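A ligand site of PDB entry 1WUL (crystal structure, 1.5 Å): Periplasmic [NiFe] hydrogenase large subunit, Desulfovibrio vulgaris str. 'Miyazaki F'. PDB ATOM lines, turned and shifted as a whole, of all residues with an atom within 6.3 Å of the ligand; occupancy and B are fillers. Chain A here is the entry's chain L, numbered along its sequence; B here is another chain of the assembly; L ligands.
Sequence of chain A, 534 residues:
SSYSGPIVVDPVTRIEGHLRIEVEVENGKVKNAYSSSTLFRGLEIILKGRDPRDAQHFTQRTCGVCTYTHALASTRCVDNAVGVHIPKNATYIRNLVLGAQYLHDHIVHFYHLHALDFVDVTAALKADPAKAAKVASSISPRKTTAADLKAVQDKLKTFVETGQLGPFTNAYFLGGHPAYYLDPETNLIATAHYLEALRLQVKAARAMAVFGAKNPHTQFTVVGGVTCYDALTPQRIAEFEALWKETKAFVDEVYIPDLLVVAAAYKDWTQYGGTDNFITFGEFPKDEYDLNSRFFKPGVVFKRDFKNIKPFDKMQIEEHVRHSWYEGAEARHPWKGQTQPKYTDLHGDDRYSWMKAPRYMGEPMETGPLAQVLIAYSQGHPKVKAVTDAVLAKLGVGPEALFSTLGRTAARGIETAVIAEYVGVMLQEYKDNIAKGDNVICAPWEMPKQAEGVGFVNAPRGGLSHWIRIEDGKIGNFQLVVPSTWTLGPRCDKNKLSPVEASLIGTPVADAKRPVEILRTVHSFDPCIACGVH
Residues that only touch the ligand: Thr 69, Ala 459, Pro 460, Leu 464, Val 482 and Pro 483. Hydrophobic or aromatic side chains that line the ligand: His 70, Ala 459, Pro 460, Leu 464, Val 482 and Pro 483. Of the 28 residues printed, 13 come within 4 Å of the ligand.
The guanidinium group of Arg 461 lies within salt-bridge range of the side-chain carboxylate of Asp 526 (2.8 Å). OE2 of Glu 16 sits at hydrogen-bond distance from OD of CSO 528, at 2.6 Å. A ring nitrogen (NE2) of His 70 sits close to the side-chain sulfur (SG) of Cys 531 (3.2 Å). The backbone carbonyl oxygen of Val 482 lies within hydrogen-bond range of the side-chain hydroxyl of Thr 485. N of CSO 528 sits at hydrogen-bond distance from the side-chain hydroxyl (OG) of Ser 484. O of Cys 66 sits at hydrogen-bond distance from OG1 of Thr 69 (2.8 Å). The backbone NH (N) of Ala 530 lies close to OD of CSO 528. The side-chain sulfur (SG) of Cys 63 lies close to the backbone NH (N) of Val 65 (3.4 Å).
The backbone NH of Arg 461 sits at hydrogen-bond distance from a nitrogen (N1) of the ligand, 2.9 Å away. N1 of the ligand lies within hydrogen-bond range of NH1 of Arg 461 (3.2 Å). A nickel atom (NI1) of the ligand is bound by the side-chain sulfur (SG) of Cys 66, at 2.2 Å. SG of Cys 531 binds FE1 of the ligand (2.3 Å). A nickel atom (NI1) of the ligand is bound by SG of CSO 528. The side-chain hydroxyl of Ser 484 is in hydrogen-bond range of an oxygen (O2) of the ligand, at 2.6 Å. N of Ser 484 is in hydrogen-bond range of O2 of the ligand (2.9 Å). The side-chain sulfur (SG) of Cys 63 binds a nickel atom (NI1) of the ligand (2.2 Å). O1 of the ligand sits close to NE2 of His 70, at 3.4 Å.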
ATOM      1  N   GLU A  16       9.868  16.105  16.624  1.00  0.00           N
ATOM      2  CA  GLU A  16      10.693  14.930  16.332  1.00  0.00           C
ATOM      3  C   GLU A  16      11.642  15.321  15.193  1.00  0.00           C
ATOM      4  O   GLU A  16      11.213  15.779  14.132  1.00  0.00           O
ATOM      5  CB  GLU A  16       9.881  13.704  15.956  1.00  0.00           C
ATOM      6  CG  GLU A  16      10.564  12.348  15.917  1.00  0.00           C
ATOM      7  CD  GLU A  16      11.621  12.154  14.829  1.00  0.00           C
ATOM      8  OE1 GLU A  16      12.723  11.646  15.016  1.00  0.00           O
ATOM      9  OE2 GLU A  16      11.337  12.811  13.758  1.00  0.00           O
ATOM     10  N   THR A  62      10.600   4.178  10.933  1.00  0.00           N
ATOM     11  CA  THR A  62      10.547   5.564  10.424  1.00  0.00           C
ATOM     12  C   THR A  62      10.430   6.567  11.566  1.00  0.00           C
ATOM     13  O   THR A  62      11.013   7.643  11.534  1.00  0.00           O
ATOM     14  CB  THR A  62       9.348   5.741   9.481  1.00  0.00           C
ATOM     15  OG1 THR A  62       9.543   4.907   8.309  1.00  0.00           O
ATOM     16  CG2 THR A  62       9.226   7.174   9.017  1.00  0.00           C
ATOM     17  N   CYS A  63       9.616   6.203  12.601  1.00  0.00           N
ATOM     18  CA  CYS A  63       9.336   7.149  13.672  1.00  0.00           C
ATOM     19  C   CYS A  63       8.873   6.451  14.932  1.00  0.00           C
ATOM     20  O   CYS A  63       7.961   5.582  14.837  1.00  0.00           O
ATOM     21  CB  CYS A  63       8.271   8.115  13.147  1.00  0.00           C
ATOM     22  SG  CYS A  63       7.961   9.436  14.385  1.00  0.00           S
ATOM     23  N   GLY A  64       9.445   6.804  16.077  1.00  0.00           N
ATOM     24  CA  GLY A  64       9.068   6.229  17.378  1.00  0.00           C
ATOM     25  C   GLY A  64       8.132   7.161  18.132  1.00  0.00           C
ATOM     26  O   GLY A  64       7.683   6.794  19.209  1.00  0.00           O
ATOM     27  N   VAL A  65       7.853   8.354  17.600  1.00  0.00           N
ATOM     28  CA  VAL A  65       6.855   9.250  18.188  1.00  0.00           C
ATOM     29  C   VAL A  65       5.514   8.775  17.682  1.00  0.00           C
ATOM     30  O   VAL A  65       4.656   8.297  18.443  1.00  0.00           O
ATOM     31  CB  VAL A  65       7.118  10.718  17.837  1.00  0.00           C
ATOM     32  CG1 VAL A  65       6.017  11.631  18.366  1.00  0.00           C
ATOM     33  CG2 VAL A  65       8.464  11.120  18.434  1.00  0.00           C
ATOM     34  N   CYS A  66       5.349   8.805  16.349  1.00  0.00           N
ATOM     35  CA  CYS A  66       4.189   8.179  15.726  1.00  0.00           C
ATOM     36  C   CYS A  66       4.526   6.709  15.505  1.00  0.00           C
ATOM     37  O   CYS A  66       4.424   6.142  14.420  1.00  0.00           O
ATOM     38  CB  CYS A  66       3.762   8.902  14.458  1.00  0.00           C
ATOM     39  SG  CYS A  66       4.954   8.882  13.095  1.00  0.00           S
ATOM     40  N   THR A  67       4.921   6.065  16.604  1.00  0.00           N
ATOM     41  CA  THR A  67       5.131   4.623  16.570  1.00  0.00           C
ATOM     42  C   THR A  67       3.811   3.956  16.165  1.00  0.00           C
ATOM     43  O   THR A  67       2.725   4.602  16.213  1.00  0.00           O
ATOM     44  CB  THR A  67       5.658   4.170  17.940  1.00  0.00           C
ATOM     45  OG1 THR A  67       6.046   2.800  17.836  1.00  0.00           O
ATOM     46  CG2 THR A  67       4.596   4.251  19.058  1.00  0.00           C
ATOM     47  N   THR A  69       2.119   3.630  13.694  1.00  0.00           N
ATOM     48  CA  THR A  69       1.431   4.096  12.492  1.00  0.00           C
ATOM     49  C   THR A  69       2.048   3.552  11.193  1.00  0.00           C
ATOM     50  O   THR A  69       1.327   3.192  10.269  1.00  0.00           O
ATOM     51  CB  THR A  69       1.388   5.644  12.403  1.00  0.00           C
ATOM     52  OG1 THR A  69       2.710   6.202  12.261  1.00  0.00           O
ATOM     53  CG2 THR A  69       0.681   6.210  13.641  1.00  0.00           C
ATOM     54  N   HIS A  70       3.381   3.447  11.139  1.00  0.00           N
ATOM     55  CA  HIS A  70       3.978   2.950   9.910  1.00  0.00           C
ATOM     56  C   HIS A  70       3.900   1.440   9.789  1.00  0.00           C
ATOM     57  O   HIS A  70       3.802   0.900   8.684  1.00  0.00           O
ATOM     58  CB  HIS A  70       5.443   3.412   9.775  1.00  0.00           C
ATOM     59  CG  HIS A  70       5.587   4.861   9.496  1.00  0.00           C
ATOM     60  ND1 HIS A  70       5.506   5.376   8.207  1.00  0.00           N
ATOM     61  CD2 HIS A  70       5.772   5.907  10.365  1.00  0.00           C
ATOM     62  CE1 HIS A  70       5.663   6.710   8.335  1.00  0.00           C
ATOM     63  NE2 HIS A  70       5.840   7.051   9.623  1.00  0.00           N
ATOM     64  N   ASP A 105      -0.127  10.581  21.637  1.00  0.00           N
ATOM     65  CA  ASP A 105       0.681  11.500  20.815  1.00  0.00           C
ATOM     66  C   ASP A 105       0.234  12.947  20.997  1.00  0.00           C
ATOM     67  O   ASP A 105       1.015  13.853  21.273  1.00  0.00           O
ATOM     68  CB  ASP A 105       0.590  10.990  19.371  1.00  0.00           C
ATOM     69  CG  ASP A 105       1.673  11.463  18.434  1.00  0.00           C
ATOM     70  OD1 ASP A 105       2.283  12.537  18.724  1.00  0.00           O
ATOM     71  OD2 ASP A 105       1.885  10.753  17.410  1.00  0.00           O
ATOM     72  N   ALA A 459      -2.688   9.372  10.306  1.00  0.00           N
ATOM     73  CA  ALA A 459      -1.876   9.322  11.511  1.00  0.00           C
ATOM     74  C   ALA A 459      -2.105  10.613  12.312  1.00  0.00           C
ATOM     75  O   ALA A 459      -2.802  11.525  11.848  1.00  0.00           O
ATOM     76  CB  ALA A 459      -0.410   9.154  11.121  1.00  0.00           C
ATOM     77  N   PRO A 460      -1.642  10.727  13.534  1.00  0.00           N
ATOM     78  CA  PRO A 460      -1.806  11.985  14.295  1.00  0.00           C
ATOM     79  C   PRO A 460      -1.344  13.225  13.534  1.00  0.00           C
ATOM     80  O   PRO A 460      -1.842  14.313  13.899  1.00  0.00           O
ATOM     81  CB  PRO A 460      -0.941  11.696  15.560  1.00  0.00           C
ATOM     82  CG  PRO A 460      -1.125  10.198  15.747  1.00  0.00           C
ATOM     83  CD  PRO A 460      -0.983   9.647  14.332  1.00  0.00           C
ATOM     84  N   ARG A 461      -0.440  13.109  12.557  1.00  0.00           N
ATOM     85  CA  ARG A 461      -0.002  14.311  11.812  1.00  0.00           C
ATOM     86  C   ARG A 461      -0.597  14.378  10.413  1.00  0.00           C
ATOM     87  O   ARG A 461      -0.305  15.307   9.671  1.00  0.00           O
ATOM     88  CB  ARG A 461       1.527  14.388  11.750  1.00  0.00           C
ATOM     89  CG  ARG A 461       2.110  14.620  13.145  1.00  0.00           C
ATOM     90  CD  ARG A 461       3.624  14.203  13.212  1.00  0.00           C
ATOM     91  NE  ARG A 461       3.999  14.430  14.606  1.00  0.00           N
ATOM     92  CZ  ARG A 461       3.718  13.561  15.588  1.00  0.00           C
ATOM     93  NH1 ARG A 461       3.145  12.367  15.347  1.00  0.00           N
ATOM     94  NH2 ARG A 461       4.046  13.881  16.837  1.00  0.00           N
ATOM     95  N   GLY A 462      -1.442  13.399  10.044  1.00  0.00           N
ATOM     96  CA  GLY A 462      -2.166  13.455   8.782  1.00  0.00           C
ATOM     97  C   GLY A 462      -2.055  12.240   7.885  1.00  0.00           C
ATOM     98  O   GLY A 462      -1.825  11.124   8.337  1.00  0.00           O
ATOM     99  N   GLY A 463      -2.266  12.479   6.586  1.00  0.00           N
ATOM    100  CA  GLY A 463      -2.427  11.392   5.636  1.00  0.00           C
ATOM    101  C   GLY A 463      -1.114  10.684   5.340  1.00  0.00           C
ATOM    102  O   GLY A 463      -0.242  11.276   4.681  1.00  0.00           O
ATOM    103  N   LEU A 464      -0.981   9.451   5.797  1.00  0.00           N
ATOM    104  CA  LEU A 464       0.161   8.574   5.564  1.00  0.00           C
ATOM    105  C   LEU A 464      -0.136   7.523   4.511  1.00  0.00           C
ATOM    106  O   LEU A 464      -1.189   6.886   4.581  1.00  0.00           O
ATOM    107  CB  LEU A 464       0.519   7.877   6.885  1.00  0.00           C
ATOM    108  CG  LEU A 464       1.573   6.758   6.833  1.00  0.00           C
ATOM    109  CD1 LEU A 464       2.910   7.273   6.290  1.00  0.00           C
ATOM    110  CD2 LEU A 464       1.724   6.125   8.208  1.00  0.00           C
ATOM    111  N   VAL A 482       4.653  10.663   3.608  1.00  0.00           N
ATOM    112  CA  VAL A 482       4.297  10.740   5.045  1.00  0.00           C
ATOM    113  C   VAL A 482       3.679  12.089   5.344  1.00  0.00           C
ATOM    114  O   VAL A 482       3.972  13.049   4.623  1.00  0.00           O
ATOM    115  CB  VAL A 482       5.589  10.444   5.839  1.00  0.00           C
ATOM    116  CG1 VAL A 482       5.389  10.332   7.328  1.00  0.00           C
ATOM    117  CG2 VAL A 482       6.211   9.119   5.398  1.00  0.00           C
ATOM    118  N   PRO A 483       2.793  12.245   6.329  1.00  0.00           N
ATOM    119  CA  PRO A 483       2.151  13.550   6.569  1.00  0.00           C
ATOM    120  C   PRO A 483       3.139  14.702   6.674  1.00  0.00           C
ATOM    121  O   PRO A 483       2.890  15.757   6.037  1.00  0.00           O
ATOM    122  CB  PRO A 483       1.344  13.366   7.861  1.00  0.00           C
ATOM    123  CG  PRO A 483       1.528  11.942   8.253  1.00  0.00           C
ATOM    124  CD  PRO A 483       2.208  11.191   7.168  1.00  0.00           C
ATOM    125  N   SER A 484       4.228  14.584   7.428  1.00  0.00           N
ATOM    126  CA  SER A 484       5.159  15.738   7.499  1.00  0.00           C
ATOM    127  C   SER A 484       5.836  16.035   6.163  1.00  0.00           C
ATOM    128  O   SER A 484       6.338  17.154   6.009  1.00  0.00           O
ATOM    129  CB  SER A 484       6.224  15.521   8.581  1.00  0.00           C
ATOM    130  OG  SER A 484       5.590  15.567   9.870  1.00  0.00           O
ATOM    131  N   THR A 485       5.879  15.018   5.279  1.00  0.00           N
ATOM    132  CA  THR A 485       6.438  15.290   3.957  1.00  0.00           C
ATOM    133  C   THR A 485       5.525  16.287   3.239  1.00  0.00           C
ATOM    134  O   THR A 485       5.978  17.266   2.645  1.00  0.00           O
ATOM    135  CB  THR A 485       6.535  14.029   3.076  1.00  0.00           C
ATOM    136  OG1 THR A 485       6.972  12.908   3.854  1.00  0.00           O
ATOM    137  CG2 THR A 485       7.483  14.275   1.922  1.00  0.00           C
ATOM    138  N   ASP A 526       3.108  20.181  14.307  1.00  0.00           N
ATOM    139  CA  ASP A 526       3.591  18.961  14.969  1.00  0.00           C
ATOM    140  C   ASP A 526       4.578  18.251  14.046  1.00  0.00           C
ATOM    141  O   ASP A 526       4.368  17.120  13.592  1.00  0.00           O
ATOM    142  CB  ASP A 526       2.386  18.107  15.354  1.00  0.00           C
ATOM    143  CG  ASP A 526       2.697  16.870  16.152  1.00  0.00           C
ATOM    144  OD1 ASP A 526       1.763  16.041  16.325  1.00  0.00           O
ATOM    145  OD2 ASP A 526       3.869  16.673  16.593  1.00  0.00           O
ATOM    146  N   PRO A 527       5.680  18.888  13.662  1.00  0.00           N
ATOM    147  CA  PRO A 527       6.604  18.303  12.674  1.00  0.00           C
ATOM    148  C   PRO A 527       7.245  17.016  13.119  1.00  0.00           C
ATOM    149  O   PRO A 527       7.632  16.852  14.284  1.00  0.00           O
ATOM    150  CB  PRO A 527       7.702  19.380  12.527  1.00  0.00           C
ATOM    151  CG  PRO A 527       7.003  20.645  12.916  1.00  0.00           C
ATOM    152  CD  PRO A 527       6.147  20.215  14.093  1.00  0.00           C
ATOM    153  N   CSO A 528       7.425  16.080  12.164  1.00  0.00           N
ATOM    154  CA  CSO A 528       8.077  14.794  12.468  1.00  0.00           C
ATOM    155  CB  CSO A 528       7.015  13.706  12.582  1.00  0.00           C
ATOM    156  SG  CSO A 528       7.618  12.294  13.533  1.00  0.00           S
ATOM    157  C   CSO A 528       9.069  14.574  11.330  1.00  0.00           C
ATOM    158  O   CSO A 528       8.639  14.195  10.247  1.00  0.00           O
ATOM    159  OD  CSO A 528       9.053  11.954  12.825  1.00  0.00           O
ATOM    160  N   ILE A 529      10.322  14.899  11.540  1.00  0.00           N
ATOM    161  CA  ILE A 529      11.252  14.968  10.393  1.00  0.00           C
ATOM    162  C   ILE A 529      11.770  13.590  10.007  1.00  0.00           C
ATOM    163  O   ILE A 529      12.077  13.348   8.830  1.00  0.00           O
ATOM    164  CB  ILE A 529      12.394  15.962  10.676  1.00  0.00           C
ATOM    165  CG1 ILE A 529      11.891  17.301  11.260  1.00  0.00           C
ATOM    166  CG2 ILE A 529      13.240  16.207   9.423  1.00  0.00           C
ATOM    167  CD1 ILE A 529      10.815  17.943  10.382  1.00  0.00           C
ATOM    168  N   ALA A 530      11.849  12.655  10.953  1.00  0.00           N
ATOM    169  CA  ALA A 530      12.206  11.262  10.668  1.00  0.00           C
ATOM    170  C   ALA A 530      11.109  10.701   9.756  1.00  0.00           C
ATOM    171  O   ALA A 530      11.345  10.017   8.751  1.00  0.00           O
ATOM    172  CB  ALA A 530      12.366  10.489  11.945  1.00  0.00           C
ATOM    173  N   CYS A 531       9.875  11.033  10.093  1.00  0.00           N
ATOM    174  CA  CYS A 531       8.729  10.718   9.231  1.00  0.00           C
ATOM    175  C   CYS A 531       8.841  11.375   7.866  1.00  0.00           C
ATOM    176  O   CYS A 531       8.667  10.740   6.816  1.00  0.00           O
ATOM    177  CB  CYS A 531       7.421  11.221   9.875  1.00  0.00           C
ATOM    178  SG  CYS A 531       6.665   9.919  10.864  1.00  0.00           S
ATOM    179  N   GLY A 532       9.079  12.692   7.829  1.00  0.00           N
ATOM    180  CA  GLY A 532       8.996  13.383   6.542  1.00  0.00           C
ATOM    181  C   GLY A 532      10.026  12.882   5.539  1.00  0.00           C
ATOM    182  O   GLY A 532       9.715  12.838   4.342  1.00  0.00           O
ATOM    183  N   CYS B  17      14.950   7.512  15.199  1.00  0.00           N
ATOM    184  CA  CYS B  17      13.520   7.665  14.958  1.00  0.00           C
ATOM    185  C   CYS B  17      12.811   8.272  16.164  1.00  0.00           C
ATOM    186  O   CYS B  17      11.607   8.514  16.103  1.00  0.00           O
ATOM    187  CB  CYS B  17      12.901   6.304  14.597  1.00  0.00           C
ATOM    188  SG  CYS B  17      12.596   5.254  16.057  1.00  0.00           S
HETATM  189 NI1  LIG L   1       6.409  10.556  13.294  1.00  0.00          NI
HETATM  190 FE1  LIG L   1       4.517  10.479  11.563  1.00  0.00          FE
HETATM  191  C1  LIG L   1       3.604   9.498  10.363  1.00  0.00           C
HETATM  192  C2  LIG L   1       2.806  11.000  12.425  1.00  0.00           C
HETATM  193  O1  LIG L   1       3.000   9.006   9.568  1.00  0.00           O
HETATM  194  N1  LIG L   1       1.743  11.193  12.769  1.00  0.00           N
HETATM  195  O2  LIG L   1       4.647  13.139   9.890  1.00  0.00           O
HETATM  196  C3  LIG L   1       4.577  12.152  10.425  1.00  0.00           C
